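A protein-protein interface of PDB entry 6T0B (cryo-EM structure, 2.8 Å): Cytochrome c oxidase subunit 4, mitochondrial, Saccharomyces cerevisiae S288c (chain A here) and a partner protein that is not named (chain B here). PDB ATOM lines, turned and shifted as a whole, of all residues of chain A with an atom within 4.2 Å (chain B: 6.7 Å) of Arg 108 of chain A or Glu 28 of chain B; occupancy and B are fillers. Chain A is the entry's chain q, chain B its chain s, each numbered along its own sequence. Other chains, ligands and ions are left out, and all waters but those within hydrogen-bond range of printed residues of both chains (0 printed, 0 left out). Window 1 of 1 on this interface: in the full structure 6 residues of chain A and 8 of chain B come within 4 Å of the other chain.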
ATOM      1  N   MET A  69      30.767   9.753  -7.416  1.00  0.00           N
ATOM      2  CA  MET A  69      30.443   8.394  -6.984  1.00  0.00           C
ATOM      3  C   MET A  69      31.550   7.397  -7.278  1.00  0.00           C
ATOM      4  O   MET A  69      31.584   6.334  -6.655  1.00  0.00           O
ATOM      5  CB  MET A  69      29.161   7.914  -7.662  1.00  0.00           C
ATOM      6  CG  MET A  69      27.911   8.645  -7.222  1.00  0.00           C
ATOM      7  SD  MET A  69      27.566   8.333  -5.486  1.00  0.00           S
ATOM      8  CE  MET A  69      27.003   6.661  -5.511  1.00  0.00           C
ATOM      9  N   LEU A  99      24.613  15.667   6.219  1.00  0.00           N
ATOM     10  CA  LEU A  99      24.341  14.338   5.701  1.00  0.00           C
ATOM     11  C   LEU A  99      24.743  13.311   6.742  1.00  0.00           C
ATOM     12  O   LEU A  99      25.488  13.605   7.677  1.00  0.00           O
ATOM     13  CB  LEU A  99      25.098  14.067   4.404  1.00  0.00           C
ATOM     14  CG  LEU A  99      24.782  14.975   3.232  1.00  0.00           C
ATOM     15  CD1 LEU A  99      25.810  14.838   2.133  1.00  0.00           C
ATOM     16  CD2 LEU A  99      23.388  14.648   2.755  1.00  0.00           C
ATOM     17  N   VAL A 106      25.684   5.478   0.931  1.00  0.00           N
ATOM     18  CA  VAL A 106      26.539   6.635   0.820  1.00  0.00           C
ATOM     19  C   VAL A 106      25.660   7.878   0.868  1.00  0.00           C
ATOM     20  O   VAL A 106      24.436   7.799   0.837  1.00  0.00           O
ATOM     21  CB  VAL A 106      27.399   6.599  -0.461  1.00  0.00           C
ATOM     22  CG1 VAL A 106      28.049   5.261  -0.605  1.00  0.00           C
ATOM     23  CG2 VAL A 106      26.559   6.894  -1.674  1.00  0.00           C
ATOM     24  N   ALA A 107      26.285   9.041   0.952  1.00  0.00           N
ATOM     25  CA  ALA A 107      25.549  10.292   1.045  1.00  0.00           C
ATOM     26  C   ALA A 107      25.746  11.110  -0.222  1.00  0.00           C
ATOM     27  O   ALA A 107      26.875  11.493  -0.538  1.00  0.00           O
ATOM     28  CB  ALA A 107      25.994  11.086   2.270  1.00  0.00           C
ATOM     29  N   ARG A 108      24.656  11.345  -0.949  1.00  0.00           N
ATOM     30  CA  ARG A 108      24.582  12.369  -1.978  1.00  0.00           C
ATOM     31  C   ARG A 108      24.235  13.693  -1.317  1.00  0.00           C
ATOM     32  O   ARG A 108      23.444  13.735  -0.377  1.00  0.00           O
ATOM     33  CB  ARG A 108      23.504  12.049  -3.016  1.00  0.00           C
ATOM     34  CG  ARG A 108      23.562  10.707  -3.750  1.00  0.00           C
ATOM     35  CD  ARG A 108      24.779  10.561  -4.602  1.00  0.00           C
ATOM     36  NE  ARG A 108      24.966  11.656  -5.544  1.00  0.00           N
ATOM     37  CZ  ARG A 108      24.778  11.558  -6.854  1.00  0.00           C
ATOM     38  NH1 ARG A 108      24.420  10.394  -7.385  1.00  0.00           N
ATOM     39  NH2 ARG A 108      24.975  12.615  -7.636  1.00  0.00           N
ATOM     40  N   CYS A 109      24.788  14.782  -1.843  1.00  0.00           N
ATOM     41  CA  CYS A 109      24.643  16.082  -1.194  1.00  0.00           C
ATOM     42  C   CYS A 109      23.356  16.806  -1.568  1.00  0.00           C
ATOM     43  O   CYS A 109      22.744  17.451  -0.706  1.00  0.00           O
ATOM     44  CB  CYS A 109      25.839  16.968  -1.530  1.00  0.00           C
ATOM     45  SG  CYS A 109      25.650  18.675  -1.016  1.00  0.00           S
ATOM     46  N   TRP A 110      22.951  16.693  -2.833  1.00  0.00           N
ATOM     47  CA  TRP A 110      21.822  17.269  -3.559  1.00  0.00           C
ATOM     48  C   TRP A 110      22.042  18.739  -3.942  1.00  0.00           C
ATOM     49  O   TRP A 110      21.385  19.215  -4.863  1.00  0.00           O
ATOM     50  CB  TRP A 110      20.468  17.096  -2.825  1.00  0.00           C
ATOM     51  CG  TRP A 110      19.291  17.789  -3.412  1.00  0.00           C
ATOM     52  CD1 TRP A 110      18.542  18.742  -2.819  1.00  0.00           C
ATOM     53  CD2 TRP A 110      18.769  17.627  -4.732  1.00  0.00           C
ATOM     54  NE1 TRP A 110      17.568  19.176  -3.672  1.00  0.00           N
ATOM     55  CE2 TRP A 110      17.689  18.505  -4.857  1.00  0.00           C
ATOM     56  CE3 TRP A 110      19.106  16.819  -5.818  1.00  0.00           C
ATOM     57  CZ2 TRP A 110      16.945  18.605  -6.020  1.00  0.00           C
ATOM     58  CZ3 TRP A 110      18.369  16.917  -6.966  1.00  0.00           C
ATOM     59  CH2 TRP A 110      17.306  17.804  -7.062  1.00  0.00           C
ATOM     60  N   GLY A 113      26.692  17.780  -4.911  1.00  0.00           N
ATOM     61  CA  GLY A 113      26.865  16.422  -5.365  1.00  0.00           C
ATOM     62  C   GLY A 113      28.081  15.708  -4.830  1.00  0.00           C
ATOM     63  O   GLY A 113      28.452  14.669  -5.378  1.00  0.00           O
ATOM     64  N   VAL A 115      29.873  13.196  -2.601  1.00  0.00           N
ATOM     65  CA  VAL A 115      29.318  11.996  -1.993  1.00  0.00           C
ATOM     66  C   VAL A 115      30.268  11.458  -0.938  1.00  0.00           C
ATOM     67  O   VAL A 115      31.487  11.651  -0.997  1.00  0.00           O
ATOM     68  CB  VAL A 115      28.993  10.950  -3.067  1.00  0.00           C
ATOM     69  CG1 VAL A 115      28.213  11.618  -4.114  1.00  0.00           C
ATOM     70  CG2 VAL A 115      30.207  10.349  -3.659  1.00  0.00           C
ATOM     71  N   GLU B  19      28.188  22.208 -17.645  1.00  0.00           N
ATOM     72  CA  GLU B  19      27.797  21.413 -16.486  1.00  0.00           C
ATOM     73  C   GLU B  19      26.732  20.376 -16.807  1.00  0.00           C
ATOM     74  O   GLU B  19      26.670  19.347 -16.132  1.00  0.00           O
ATOM     75  CB  GLU B  19      27.309  22.309 -15.356  1.00  0.00           C
ATOM     76  CG  GLU B  19      27.505  21.678 -14.005  1.00  0.00           C
ATOM     77  CD  GLU B  19      27.068  22.559 -12.867  1.00  0.00           C
ATOM     78  OE1 GLU B  19      26.589  23.679 -13.125  1.00  0.00           O
ATOM     79  OE2 GLU B  19      27.205  22.126 -11.705  1.00  0.00           O
ATOM     80  N   PHE B  20      25.914  20.599 -17.830  1.00  0.00           N
ATOM     81  CA  PHE B  20      24.987  19.555 -18.234  1.00  0.00           C
ATOM     82  C   PHE B  20      25.684  18.440 -18.992  1.00  0.00           C
ATOM     83  O   PHE B  20      25.294  17.276 -18.860  1.00  0.00           O
ATOM     84  CB  PHE B  20      23.866  20.136 -19.076  1.00  0.00           C
ATOM     85  CG  PHE B  20      22.676  20.528 -18.283  1.00  0.00           C
ATOM     86  CD1 PHE B  20      21.843  19.571 -17.754  1.00  0.00           C
ATOM     87  CD2 PHE B  20      22.397  21.854 -18.052  1.00  0.00           C
ATOM     88  CE1 PHE B  20      20.747  19.934 -17.016  1.00  0.00           C
ATOM     89  CE2 PHE B  20      21.303  22.222 -17.317  1.00  0.00           C
ATOM     90  CZ  PHE B  20      20.479  21.262 -16.799  1.00  0.00           C
ATOM     91  N   GLU B  22      28.681  17.542 -18.326  1.00  0.00           N
ATOM     92  CA  GLU B  22      29.415  16.833 -17.282  1.00  0.00           C
ATOM     93  C   GLU B  22      28.459  16.274 -16.227  1.00  0.00           C
ATOM     94  O   GLU B  22      28.523  16.603 -15.046  1.00  0.00           O
ATOM     95  CB  GLU B  22      30.455  17.749 -16.657  1.00  0.00           C
ATOM     96  CG  GLU B  22      31.641  18.002 -17.551  1.00  0.00           C
ATOM     97  CD  GLU B  22      32.482  16.762 -17.776  1.00  0.00           C
ATOM     98  OE1 GLU B  22      32.619  15.958 -16.833  1.00  0.00           O
ATOM     99  OE2 GLU B  22      32.997  16.584 -18.901  1.00  0.00           O
ATOM    100  N   ALA B  23      27.557  15.407 -16.678  1.00  0.00           N
ATOM    101  CA  ALA B  23      26.677  14.658 -15.795  1.00  0.00           C
ATOM    102  C   ALA B  23      26.862  13.170 -16.047  1.00  0.00           C
ATOM    103  O   ALA B  23      27.319  12.754 -17.113  1.00  0.00           O
ATOM    104  CB  ALA B  23      25.213  15.053 -15.997  1.00  0.00           C
ATOM    105  N   TYR B  24      26.528  12.358 -15.048  1.00  0.00           N
ATOM    106  CA  TYR B  24      26.740  10.924 -15.188  1.00  0.00           C
ATOM    107  C   TYR B  24      25.610  10.053 -14.678  1.00  0.00           C
ATOM    108  O   TYR B  24      25.578   8.873 -15.032  1.00  0.00           O
ATOM    109  CB  TYR B  24      28.038  10.505 -14.493  1.00  0.00           C
ATOM    110  CG  TYR B  24      28.108  10.803 -13.011  1.00  0.00           C
ATOM    111  CD1 TYR B  24      28.575  12.022 -12.549  1.00  0.00           C
ATOM    112  CD2 TYR B  24      27.742   9.849 -12.074  1.00  0.00           C
ATOM    113  CE1 TYR B  24      28.649  12.293 -11.203  1.00  0.00           C
ATOM    114  CE2 TYR B  24      27.812  10.113 -10.726  1.00  0.00           C
ATOM    115  CZ  TYR B  24      28.263  11.336 -10.299  1.00  0.00           C
ATOM    116  OH  TYR B  24      28.336  11.596  -8.952  1.00  0.00           O
ATOM    117  N   ASP B  25      24.689  10.552 -13.868  1.00  0.00           N
ATOM    118  CA  ASP B  25      23.575   9.736 -13.417  1.00  0.00           C
ATOM    119  C   ASP B  25      22.356  10.624 -13.245  1.00  0.00           C
ATOM    120  O   ASP B  25      22.404  11.837 -13.467  1.00  0.00           O
ATOM    121  CB  ASP B  25      23.897   8.988 -12.127  1.00  0.00           C
ATOM    122  CG  ASP B  25      24.101   9.912 -10.957  1.00  0.00           C
ATOM    123  OD1 ASP B  25      24.670  10.998 -11.155  1.00  0.00           O
ATOM    124  OD2 ASP B  25      23.698   9.550  -9.835  1.00  0.00           O
ATOM    125  N   LEU B  26      21.250   9.999 -12.853  1.00  0.00           N
ATOM    126  CA  LEU B  26      19.972  10.687 -12.855  1.00  0.00           C
ATOM    127  C   LEU B  26      19.847  11.649 -11.688  1.00  0.00           C
ATOM    128  O   LEU B  26      19.058  12.592 -11.760  1.00  0.00           O
ATOM    129  CB  LEU B  26      18.863   9.647 -12.840  1.00  0.00           C
ATOM    130  CG  LEU B  26      17.458  10.043 -13.259  1.00  0.00           C
ATOM    131  CD1 LEU B  26      16.815   8.848 -13.889  1.00  0.00           C
ATOM    132  CD2 LEU B  26      16.635  10.446 -12.093  1.00  0.00           C
ATOM    133  N   PHE B  27      20.601  11.425 -10.620  1.00  0.00           N
ATOM    134  CA  PHE B  27      20.713  12.427  -9.574  1.00  0.00           C
ATOM    135  C   PHE B  27      21.384  13.680 -10.101  1.00  0.00           C
ATOM    136  O   PHE B  27      21.008  14.797  -9.726  1.00  0.00           O
ATOM    137  CB  PHE B  27      21.501  11.857  -8.404  1.00  0.00           C
ATOM    138  CG  PHE B  27      21.313  12.597  -7.119  1.00  0.00           C
ATOM    139  CD1 PHE B  27      22.027  13.744  -6.846  1.00  0.00           C
ATOM    140  CD2 PHE B  27      20.436  12.120  -6.167  1.00  0.00           C
ATOM    141  CE1 PHE B  27      21.856  14.401  -5.671  1.00  0.00           C
ATOM    142  CE2 PHE B  27      20.259  12.786  -4.980  1.00  0.00           C
ATOM    143  CZ  PHE B  27      20.965  13.926  -4.734  1.00  0.00           C
ATOM    144  N   GLU B  28      22.365  13.522 -10.982  1.00  0.00           N
ATOM    145  CA  GLU B  28      23.152  14.675 -11.381  1.00  0.00           C
ATOM    146  C   GLU B  28      22.408  15.568 -12.358  1.00  0.00           C
ATOM    147  O   GLU B  28      22.496  16.791 -12.250  1.00  0.00           O
ATOM    148  CB  GLU B  28      24.483  14.234 -11.959  1.00  0.00           C
ATOM    149  CG  GLU B  28      25.546  14.132 -10.899  1.00  0.00           C
ATOM    150  CD  GLU B  28      25.711  15.414 -10.123  1.00  0.00           C
ATOM    151  OE1 GLU B  28      26.248  16.385 -10.693  1.00  0.00           O
ATOM    152  OE2 GLU B  28      25.302  15.459  -8.944  1.00  0.00           O
ATOM    153  N   VAL B  29      21.651  15.001 -13.297  1.00  0.00           N
ATOM    154  CA  VAL B  29      20.948  15.878 -14.228  1.00  0.00           C
ATOM    155  C   VAL B  29      19.733  16.509 -13.553  1.00  0.00           C
ATOM    156  O   VAL B  29      19.408  17.677 -13.808  1.00  0.00           O
ATOM    157  CB  VAL B  29      20.610  15.130 -15.534  1.00  0.00           C
ATOM    158  CG1 VAL B  29      19.659  13.971 -15.301  1.00  0.00           C
ATOM    159  CG2 VAL B  29      20.068  16.083 -16.577  1.00  0.00           C
ATOM    160  N   GLN B  30      19.121  15.806 -12.600  1.00  0.00           N
ATOM    161  CA  GLN B  30      18.063  16.396 -11.799  1.00  0.00           C
ATOM    162  C   GLN B  30      18.592  17.384 -10.782  1.00  0.00           C
ATOM    163  O   GLN B  30      17.810  18.143 -10.209  1.00  0.00           O
ATOM    164  CB  GLN B  30      17.285  15.316 -11.068  1.00  0.00           C
ATOM    165  CG  GLN B  30      16.184  14.709 -11.862  1.00  0.00           C
ATOM    166  CD  GLN B  30      15.521  13.614 -11.099  1.00  0.00           C
ATOM    167  OE1 GLN B  30      16.024  13.195 -10.067  1.00  0.00           O
ATOM    168  NE2 GLN B  30      14.398  13.126 -11.596  1.00  0.00           N
ATOM    169  N   ARG B  31      19.888  17.382 -10.523  1.00  0.00           N
ATOM    170  CA  ARG B  31      20.440  18.417  -9.668  1.00  0.00           C
ATOM    171  C   ARG B  31      20.846  19.638 -10.481  1.00  0.00           C
ATOM    172  O   ARG B  31      20.607  20.778 -10.062  1.00  0.00           O
ATOM    173  CB  ARG B  31      21.626  17.867  -8.892  1.00  0.00           C
ATOM    174  CG  ARG B  31      22.261  18.854  -7.969  1.00  0.00           C
ATOM    175  CD  ARG B  31      23.534  18.290  -7.410  1.00  0.00           C
ATOM    176  NE  ARG B  31      24.547  18.170  -8.444  1.00  0.00           N
ATOM    177  CZ  ARG B  31      25.376  19.148  -8.780  1.00  0.00           C
ATOM    178  NH1 ARG B  31      26.272  18.962  -9.736  1.00  0.00           N
ATOM    179  NH2 ARG B  31      25.314  20.310  -8.153  1.00  0.00           N
ATOM    180  N   VAL B  32      21.454  19.416 -11.649  1.00  0.00           N
ATOM    181  CA  VAL B  32      21.930  20.517 -12.475  1.00  0.00           C
ATOM    182  C   VAL B  32      20.758  21.285 -13.075  1.00  0.00           C
ATOM    183  O   VAL B  32      20.821  22.518 -13.201  1.00  0.00           O
ATOM    184  CB  VAL B  32      22.909  19.966 -13.527  1.00  0.00           C
ATOM    185  CG1 VAL B  32      23.257  20.983 -14.571  1.00  0.00           C
ATOM    186  CG2 VAL B  32      24.183  19.515 -12.856  1.00  0.00           C
ATOM    187  N   LEU B  33      19.633  20.612 -13.336  1.00  0.00           N
ATOM    188  CA  LEU B  33      18.462  21.327 -13.826  1.00  0.00           C
ATOM    189  C   LEU B  33      17.852  22.187 -12.733  1.00  0.00           C
ATOM    190  O   LEU B  33      17.427  23.315 -12.999  1.00  0.00           O
ATOM    191  CB  LEU B  33      17.435  20.337 -14.347  1.00  0.00           C
ATOM    192  CG  LEU B  33      16.439  20.756 -15.411  1.00  0.00           C
ATOM    193  CD1 LEU B  33      15.986  19.487 -16.005  1.00  0.00           C
ATOM    194  CD2 LEU B  33      15.296  21.548 -14.944  1.00  0.00           C
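OH of Tyr 24 of chain B is in hydrogen-bond range of N of Met 69 of chain A (3.4 Å). The side-chain carboxylate (OD2) of Asp 25 of chain B lies within salt-bridge range of the guanidinium group (NH1) of Arg 108 of chain A, at 2.7 Å. NH2 of Arg 108 of chain A lies within salt-bridge range of OE2 of Glu 28 of chain B (3.1 Å).
OE2 of Glu 19 of chain B lies within salt-bridge range of NH1 of Arg 31 of chain B (3.8 Å). The side-chain carboxylate (OD1) of Asp 25 of chain B sits close to the backbone NH (N) of Glu 28 of chain B (3.4 Å). The guanidinium group (NH1) of Arg 31 of chain B lies within salt-bridge range of the side-chain carboxylate (OE1) of Glu 28 of chain B (2.7 Å).
Among the printed residues, merely in contact across the chains: Trp 110 of chain A with Gln 30 of chain B, Trp 110 of chain A with Arg 31 of chain B, Arg 108 of chain A with Phe 27 of chain B, Trp 110 of chain A with Phe 27 of chain B and Arg 108 of chain A with Tyr 24 of chain B.
Of the printed residues of chain B, Met 69 of chain A touches Tyr 24 (3.4 Å). Arg 108 of chain A touches four residues of chain B. Of the printed residues of chain A, Tyr 24 of chain B touches Met 69 and Arg 108. Printed residues of chain A within 4 Å of Asp 25 of chain B: Arg 108. Of the printed residues of chain A, Phe 27 of chain B touches Arg 108 (3.3 Å) and Trp 110 (3.6 Å). Printed residues of chain A within 4 Å of Glu 28 of chain B: Arg 108 (3.1 Å). Of the printed residues of chain A, Gln 30 of chain B touches Trp 110 (3.2 Å). The nearest residue of chain B that does not touch Arg 108 of chain A is Arg 31 of chain B (5.6 Å). The nearest residue of chain A that does not touch Glu 28 of chain B is Gly 113 of chain A (4.02 Å).
Printed residues of chain A that touch a printed residue of chain B: Met 69, Arg 108 and Trp 110. Hydrophobic or aromatic side chains of chain A that line the printed part of chain B: Met 69 and Trp 110. Of the 14 printed residues of chain B, 6 touch a printed residue of chain A. Among the printed residues, 8 pairs touch across the chains. Among the printed residues, Asp or Glu carboxylates within 4 Å of a Lys or Arg side-chain nitrogen of the other chain: Arg 108 of chain A with Asp 25 of chain B and Arg 108 of chain A with Glu 28 of chain B.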
